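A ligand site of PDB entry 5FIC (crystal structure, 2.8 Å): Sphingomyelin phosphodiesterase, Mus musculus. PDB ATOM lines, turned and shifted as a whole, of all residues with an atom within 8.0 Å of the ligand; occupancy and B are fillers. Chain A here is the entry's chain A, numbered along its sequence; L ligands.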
ATOM      1  N   ALA A  16     -18.920  13.000   7.721  1.00  0.00           N
ATOM      2  CA  ALA A  16     -17.752  12.176   7.997  1.00  0.00           C
ATOM      3  C   ALA A  16     -16.509  12.740   7.320  1.00  0.00           C
ATOM      4  O   ALA A  16     -15.426  12.738   7.897  1.00  0.00           O
ATOM      5  CB  ALA A  16     -18.001  10.736   7.540  1.00  0.00           C
ATOM      6  N   CYS A  17     -16.668  13.211   6.086  1.00  0.00           N
ATOM      7  CA  CYS A  17     -15.569  13.904   5.406  1.00  0.00           C
ATOM      8  C   CYS A  17     -15.107  15.102   6.218  1.00  0.00           C
ATOM      9  O   CYS A  17     -13.914  15.220   6.544  1.00  0.00           O
ATOM     10  CB  CYS A  17     -16.017  14.323   4.004  1.00  0.00           C
ATOM     11  SG  CYS A  17     -14.818  15.345   3.106  1.00  0.00           S
ATOM     12  N   VAL A  19     -15.387  15.835   9.266  1.00  0.00           N
ATOM     13  CA  VAL A  19     -14.808  15.481  10.566  1.00  0.00           C
ATOM     14  C   VAL A  19     -13.375  14.979  10.393  1.00  0.00           C
ATOM     15  O   VAL A  19     -12.447  15.475  11.037  1.00  0.00           O
ATOM     16  CB  VAL A  19     -15.681  14.431  11.275  1.00  0.00           C
ATOM     17  CG1 VAL A  19     -14.949  13.851  12.495  1.00  0.00           C
ATOM     18  CG2 VAL A  19     -17.003  15.049  11.689  1.00  0.00           C
ATOM     19  N   LEU A  20     -13.195  13.969   9.551  1.00  0.00           N
ATOM     20  CA  LEU A  20     -11.891  13.347   9.391  1.00  0.00           C
ATOM     21  C   LEU A  20     -10.827  14.374   9.040  1.00  0.00           C
ATOM     22  O   LEU A  20      -9.777  14.437   9.680  1.00  0.00           O
ATOM     23  CB  LEU A  20     -11.992  12.258   8.323  1.00  0.00           C
ATOM     24  CG  LEU A  20     -10.719  11.449   8.049  1.00  0.00           C
ATOM     25  CD1 LEU A  20     -10.201  10.781   9.309  1.00  0.00           C
ATOM     26  CD2 LEU A  20     -11.000  10.418   6.969  1.00  0.00           C
ATOM     27  N   PHE A  21     -11.086  15.188   8.020  1.00  0.00           N
ATOM     28  CA  PHE A  21     -10.105  16.192   7.608  1.00  0.00           C
ATOM     29  C   PHE A  21      -9.761  17.134   8.740  1.00  0.00           C
ATOM     30  O   PHE A  21      -8.613  17.570   8.872  1.00  0.00           O
ATOM     31  CB  PHE A  21     -10.630  16.976   6.403  1.00  0.00           C
ATOM     32  CG  PHE A  21     -10.573  16.211   5.110  1.00  0.00           C
ATOM     33  CD1 PHE A  21      -9.446  15.474   4.771  1.00  0.00           C
ATOM     34  CD2 PHE A  21     -11.640  16.228   4.229  1.00  0.00           C
ATOM     35  CE1 PHE A  21      -9.392  14.774   3.581  1.00  0.00           C
ATOM     36  CE2 PHE A  21     -11.587  15.517   3.053  1.00  0.00           C
ATOM     37  CZ  PHE A  21     -10.455  14.791   2.723  1.00  0.00           C
ATOM     38  N   THR A  22     -10.746  17.464   9.579  1.00  0.00           N
ATOM     39  CA  THR A  22     -10.470  18.321  10.726  1.00  0.00           C
ATOM     40  C   THR A  22      -9.460  17.664  11.655  1.00  0.00           C
ATOM     41  O   THR A  22      -8.528  18.330  12.131  1.00  0.00           O
ATOM     42  CB  THR A  22     -11.777  18.613  11.473  1.00  0.00           C
ATOM     43  OG1 THR A  22     -12.743  19.142  10.549  1.00  0.00           O
ATOM     44  CG2 THR A  22     -11.534  19.620  12.582  1.00  0.00           C
ATOM     45  N   ALA A  23      -9.618  16.365  11.925  1.00  0.00           N
ATOM     46  CA  ALA A  23      -8.711  15.693  12.833  1.00  0.00           C
ATOM     47  C   ALA A  23      -7.292  15.669  12.301  1.00  0.00           C
ATOM     48  O   ALA A  23      -6.332  16.024  12.997  1.00  0.00           O
ATOM     49  CB  ALA A  23      -9.211  14.269  13.102  1.00  0.00           C
ATOM     50  N   LEU A  24      -7.125  15.261  11.035  1.00  0.00           N
ATOM     51  CA  LEU A  24      -5.795  15.184  10.446  1.00  0.00           C
ATOM     52  C   LEU A  24      -5.101  16.536  10.482  1.00  0.00           C
ATOM     53  O   LEU A  24      -3.912  16.625  10.799  1.00  0.00           O
ATOM     54  CB  LEU A  24      -5.885  14.666   9.013  1.00  0.00           C
ATOM     55  CG  LEU A  24      -6.609  13.329   8.810  1.00  0.00           C
ATOM     56  CD1 LEU A  24      -6.532  12.935   7.348  1.00  0.00           C
ATOM     57  CD2 LEU A  24      -6.028  12.234   9.682  1.00  0.00           C
ATOM     58  N   ASN A  25      -5.843  17.604  10.152  1.00  0.00           N
ATOM     59  CA  ASN A  25      -5.250  18.938  10.203  1.00  0.00           C
ATOM     60  C   ASN A  25      -4.734  19.258  11.598  1.00  0.00           C
ATOM     61  O   ASN A  25      -3.673  19.867  11.758  1.00  0.00           O
ATOM     62  CB  ASN A  25      -6.281  19.971   9.757  1.00  0.00           C
ATOM     63  CG  ASN A  25      -6.705  19.791   8.302  1.00  0.00           C
ATOM     64  OD1 ASN A  25      -5.945  19.263   7.488  1.00  0.00           O
ATOM     65  ND2 ASN A  25      -7.908  20.244   7.979  1.00  0.00           N
ATOM     66  N   HIS A  26      -5.482  18.853  12.624  1.00  0.00           N
ATOM     67  CA  HIS A  26      -5.013  19.060  13.993  1.00  0.00           C
ATOM     68  C   HIS A  26      -3.801  18.188  14.286  1.00  0.00           C
ATOM     69  O   HIS A  26      -2.821  18.650  14.877  1.00  0.00           O
ATOM     70  CB  HIS A  26      -6.142  18.760  14.985  1.00  0.00           C
ATOM     71  CG  HIS A  26      -7.335  19.647  14.817  1.00  0.00           C
ATOM     72  ND1 HIS A  26      -7.464  20.523  13.760  1.00  0.00           N
ATOM     73  CD2 HIS A  26      -8.453  19.783  15.557  1.00  0.00           C
ATOM     74  CE1 HIS A  26      -8.620  21.169  13.868  1.00  0.00           C
ATOM     75  NE2 HIS A  26      -9.236  20.731  14.944  1.00  0.00           N
ATOM     76  N   GLY A  27      -3.846  16.910  13.885  1.00  0.00           N
ATOM     77  CA  GLY A  27      -2.707  16.038  14.083  1.00  0.00           C
ATOM     78  C   GLY A  27      -1.454  16.503  13.373  1.00  0.00           C
ATOM     79  O   GLY A  27      -0.350  16.121  13.759  1.00  0.00           O
ATOM     80  N   LEU A  28      -1.614  17.306  12.315  1.00  0.00           N
ATOM     81  CA  LEU A  28      -0.466  17.854  11.611  1.00  0.00           C
ATOM     82  C   LEU A  28       0.081  19.094  12.293  1.00  0.00           C
ATOM     83  O   LEU A  28       1.169  19.550  11.926  1.00  0.00           O
ATOM     84  CB  LEU A  28      -0.853  18.168  10.175  1.00  0.00           C
ATOM     85  CG  LEU A  28      -1.087  16.897   9.352  1.00  0.00           C
ATOM     86  CD1 LEU A  28      -1.944  17.177   8.141  1.00  0.00           C
ATOM     87  CD2 LEU A  28       0.242  16.289   8.932  1.00  0.00           C
ATOM     88  N   LYS A  29      -0.631  19.658  13.272  1.00  0.00           N
ATOM     89  CA  LYS A  29      -0.015  20.642  14.155  1.00  0.00           C
ATOM     90  C   LYS A  29       1.183  20.029  14.875  1.00  0.00           C
ATOM     91  O   LYS A  29       2.193  20.703  15.075  1.00  0.00           O
ATOM     92  CB  LYS A  29      -1.048  21.141  15.169  1.00  0.00           C
ATOM     93  CG  LYS A  29      -2.321  21.703  14.559  1.00  0.00           C
ATOM     94  CD  LYS A  29      -2.030  22.806  13.567  1.00  0.00           C
ATOM     95  CE  LYS A  29      -3.260  23.664  13.314  1.00  0.00           C
ATOM     96  NZ  LYS A  29      -3.575  23.784  11.862  1.00  0.00           N
ATOM     97  N   LYS A  30       1.074  18.758  15.259  1.00  0.00           N
ATOM     98  CA  LYS A  30       2.150  18.077  15.959  1.00  0.00           C
ATOM     99  C   LYS A  30       3.187  17.608  14.954  1.00  0.00           C
ATOM    100  O   LYS A  30       2.895  16.777  14.085  1.00  0.00           O
ATOM    101  CB  LYS A  30       1.586  16.913  16.771  1.00  0.00           C
ATOM    102  CG  LYS A  30       0.448  17.308  17.702  1.00  0.00           C
ATOM    103  CD  LYS A  30      -0.172  16.116  18.405  1.00  0.00           C
ATOM    104  CE  LYS A  30       0.725  15.564  19.498  1.00  0.00           C
ATOM    105  NZ  LYS A  30       0.063  14.465  20.259  1.00  0.00           N
ATOM    106  N   ASN A  33       4.164  13.645  13.675  1.00  0.00           N
ATOM    107  CA  ASN A  33       3.430  13.106  12.540  1.00  0.00           C
ATOM    108  C   ASN A  33       3.903  13.756  11.244  1.00  0.00           C
ATOM    109  O   ASN A  33       4.182  13.072  10.247  1.00  0.00           O
ATOM    110  CB  ASN A  33       1.927  13.322  12.730  1.00  0.00           C
ATOM    111  CG  ASN A  33       1.413  12.680  14.006  1.00  0.00           C
ATOM    112  OD1 ASN A  33       1.955  11.673  14.465  1.00  0.00           O
ATOM    113  ND2 ASN A  33       0.360  13.250  14.580  1.00  0.00           N
ATOM    114  N   VAL A  34       4.004  15.088  11.234  1.00  0.00           N
ATOM    115  CA  VAL A  34       4.535  15.796  10.071  1.00  0.00           C
ATOM    116  C   VAL A  34       5.897  15.238   9.700  1.00  0.00           C
ATOM    117  O   VAL A  34       6.205  15.037   8.514  1.00  0.00           O
ATOM    118  CB  VAL A  34       4.608  17.302  10.360  1.00  0.00           C
ATOM    119  CG1 VAL A  34       5.185  18.044   9.161  1.00  0.00           C
ATOM    120  CG2 VAL A  34       3.235  17.850  10.713  1.00  0.00           C
ATOM    121  N   ARG A  36       6.911  12.195  10.185  1.00  0.00           N
ATOM    122  CA  ARG A  36       6.575  10.972   9.466  1.00  0.00           C
ATOM    123  C   ARG A  36       6.092  11.288   8.054  1.00  0.00           C
ATOM    124  O   ARG A  36       6.549  10.696   7.070  1.00  0.00           O
ATOM    125  CB  ARG A  36       5.523  10.177  10.224  1.00  0.00           C
ATOM    126  CG  ARG A  36       5.965   9.690  11.593  1.00  0.00           C
ATOM    127  CD  ARG A  36       4.851   8.954  12.297  1.00  0.00           C
ATOM    128  NE  ARG A  36       5.211   8.551  13.653  1.00  0.00           N
ATOM    129  CZ  ARG A  36       4.384   7.959  14.501  1.00  0.00           C
ATOM    130  NH1 ARG A  36       3.142   7.678  14.138  1.00  0.00           N
ATOM    131  NH2 ARG A  36       4.800   7.638  15.712  1.00  0.00           N
ATOM    132  N   VAL A  37       5.152  12.230   7.942  1.00  0.00           N
ATOM    133  CA  VAL A  37       4.698  12.674   6.634  1.00  0.00           C
ATOM    134  C   VAL A  37       5.867  13.208   5.825  1.00  0.00           C
ATOM    135  O   VAL A  37       5.928  13.022   4.601  1.00  0.00           O
ATOM    136  CB  VAL A  37       3.582  13.721   6.785  1.00  0.00           C
ATOM    137  CG1 VAL A  37       3.112  14.197   5.412  1.00  0.00           C
ATOM    138  CG2 VAL A  37       2.417  13.158   7.578  1.00  0.00           C
ATOM    139  N   VAL A  40       7.957  10.318   4.347  1.00  0.00           N
ATOM    140  CA  VAL A  40       7.407   9.736   3.131  1.00  0.00           C
ATOM    141  C   VAL A  40       7.870  10.522   1.907  1.00  0.00           C
ATOM    142  O   VAL A  40       8.373   9.953   0.937  1.00  0.00           O
ATOM    143  CB  VAL A  40       5.864   9.682   3.215  1.00  0.00           C
ATOM    144  CG1 VAL A  40       5.287   9.082   1.945  1.00  0.00           C
ATOM    145  CG2 VAL A  40       5.424   8.889   4.435  1.00  0.00           C
ATOM    146  N   VAL A  68       2.865  21.645   4.636  1.00  0.00           N
ATOM    147  CA  VAL A  68       1.739  21.117   5.386  1.00  0.00           C
ATOM    148  C   VAL A  68       0.799  22.234   5.805  1.00  0.00           C
ATOM    149  O   VAL A  68      -0.426  22.043   5.871  1.00  0.00           O
ATOM    150  CB  VAL A  68       2.245  20.300   6.593  1.00  0.00           C
ATOM    151  CG1 VAL A  68       1.129  20.022   7.588  1.00  0.00           C
ATOM    152  CG2 VAL A  68       2.863  18.993   6.109  1.00  0.00           C
ATOM    153  N   TRP A  71      -1.494  23.037   2.884  1.00  0.00           N
ATOM    154  CA  TRP A  71      -2.382  21.900   2.694  1.00  0.00           C
ATOM    155  C   TRP A  71      -3.566  21.969   3.650  1.00  0.00           C
ATOM    156  O   TRP A  71      -4.726  21.806   3.247  1.00  0.00           O
ATOM    157  CB  TRP A  71      -1.594  20.601   2.887  1.00  0.00           C
ATOM    158  CG  TRP A  71      -0.730  20.248   1.725  1.00  0.00           C
ATOM    159  CD1 TRP A  71      -0.761  20.779   0.467  1.00  0.00           C
ATOM    160  CD2 TRP A  71       0.315  19.259   1.705  1.00  0.00           C
ATOM    161  NE1 TRP A  71       0.186  20.193  -0.327  1.00  0.00           N
ATOM    162  CE2 TRP A  71       0.867  19.262   0.403  1.00  0.00           C
ATOM    163  CE3 TRP A  71       0.835  18.386   2.661  1.00  0.00           C
ATOM    164  CZ2 TRP A  71       1.903  18.410   0.047  1.00  0.00           C
ATOM    165  CZ3 TRP A  71       1.870  17.554   2.305  1.00  0.00           C
ATOM    166  CH2 TRP A  71       2.394  17.564   1.001  1.00  0.00           C
ATOM    167  N   LEU A  76      -6.751  20.188   1.803  1.00  0.00           N
ATOM    168  CA  LEU A  76      -7.384  19.322   2.781  1.00  0.00           C
ATOM    169  C   LEU A  76      -8.316  20.073   3.715  1.00  0.00           C
ATOM    170  O   LEU A  76      -8.804  19.499   4.692  1.00  0.00           O
ATOM    171  CB  LEU A  76      -6.320  18.556   3.568  1.00  0.00           C
ATOM    172  CG  LEU A  76      -5.525  17.571   2.703  1.00  0.00           C
ATOM    173  CD1 LEU A  76      -4.317  18.239   2.078  1.00  0.00           C
ATOM    174  CD2 LEU A  76      -5.090  16.348   3.499  1.00  0.00           C
ATOM    175  N   ALA A  81     -12.120  19.967   0.161  1.00  0.00           N
ATOM    176  CA  ALA A  81     -11.933  18.560  -0.140  1.00  0.00           C
ATOM    177  C   ALA A  81     -13.270  17.842  -0.326  1.00  0.00           C
ATOM    178  O   ALA A  81     -13.468  17.124  -1.320  1.00  0.00           O
ATOM    179  CB  ALA A  81     -11.117  17.891   0.965  1.00  0.00           C
ATOM    180  N   LEU A  85     -14.852  15.293  -3.653  1.00  0.00           N
ATOM    181  CA  LEU A  85     -15.189  13.874  -3.648  1.00  0.00           C
ATOM    182  C   LEU A  85     -16.682  13.656  -3.818  1.00  0.00           C
ATOM    183  O   LEU A  85     -17.103  12.727  -4.523  1.00  0.00           O
ATOM    184  CB  LEU A  85     -14.714  13.231  -2.342  1.00  0.00           C
ATOM    185  CG  LEU A  85     -13.198  13.062  -2.214  1.00  0.00           C
ATOM    186  CD1 LEU A  85     -12.813  12.867  -0.764  1.00  0.00           C
ATOM    187  CD2 LEU A  85     -12.736  11.871  -3.046  1.00  0.00           C
HETATM  188  C1  LIG L   1      -2.694  12.862  11.117  1.00  0.00           C
HETATM  189  C2  LIG L   1      -3.559  11.973  12.021  1.00  0.00           C
HETATM  190  C3  LIG L   1      -4.283  12.783  13.085  1.00  0.00           C
HETATM  191  C4  LIG L   1      -5.023  11.927  14.107  1.00  0.00           C
HETATM  192  C5  LIG L   1     -10.365   9.105   3.561  1.00  0.00           C
HETATM  193  C6  LIG L   1     -10.029  10.125   2.484  1.00  0.00           C
HETATM  194  C7  LIG L   1      -9.026   9.574   1.456  1.00  0.00           C
HETATM  195  C8  LIG L   1      -7.948  10.584   1.055  1.00  0.00           C
HETATM  196  C9  LIG L   1      -7.181  11.131   2.267  1.00  0.00           C
HETATM  197  C10 LIG L   1      -5.740  11.539   1.970  1.00  0.00           C
HETATM  198  C11 LIG L   1      -5.131  12.339   3.112  1.00  0.00           C
HETATM  199  C12 LIG L   1      -3.775  11.791   3.570  1.00  0.00           C
HETATM  200  C13 LIG L   1      -3.018  12.764   4.469  1.00  0.00           C
HETATM  201  C14 LIG L   1      -2.602  12.116   5.797  1.00  0.00           C
HETATM  202  C15 LIG L   1      -1.408  12.801   6.448  1.00  0.00           C
HETATM  203  C16 LIG L   1      -0.983  12.086   7.730  1.00  0.00           C
HETATM  204  C17 LIG L   1      -1.296  12.885   8.993  1.00  0.00           C
HETATM  205  C18 LIG L   1      -2.049  12.028  10.014  1.00  0.00           C
HETATM  206  P1  LIG L   1      -5.355  12.912  15.650  1.00  0.00           P
HETATM  207  O1  LIG L   1      -4.151  12.987  16.475  1.00  0.00           O
HETATM  208  O2  LIG L   1      -6.574  12.181  16.499  1.00  0.00           O
HETATM  209  O3  LIG L   1      -5.809  14.446  15.233  1.00  0.00           O
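An oxygen (O3) of the ligand lies close to the backbone carbonyl oxygen (O) of Ala 23 (2.8 Å).
The backbone NH (N) of Gly 27 is in hydrogen-bond range of an oxygen (O3) of the ligand (3.4 Å).
The side-chain amide nitrogen of Asn 33 is in hydrogen-bond range of the backbone carbonyl oxygen of Gly 27.
CD2 of Leu 20 touches C5 of the ligand, 3.7 Å away.
Leu 24 touches the ligand.
Leu 28 touches the ligand (CD2 to C17, 3.7 Å).
Val 37 touches the ligand.
Hydrophobic or aromatic side chains within 4 Å of the ligand: Leu 20, Leu 24, Leu 28 and Val 37.
Within 4 Å of the ligand: Leu 20, Ala 23, Leu 24, Gly 27, Leu 28 and Val 37.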
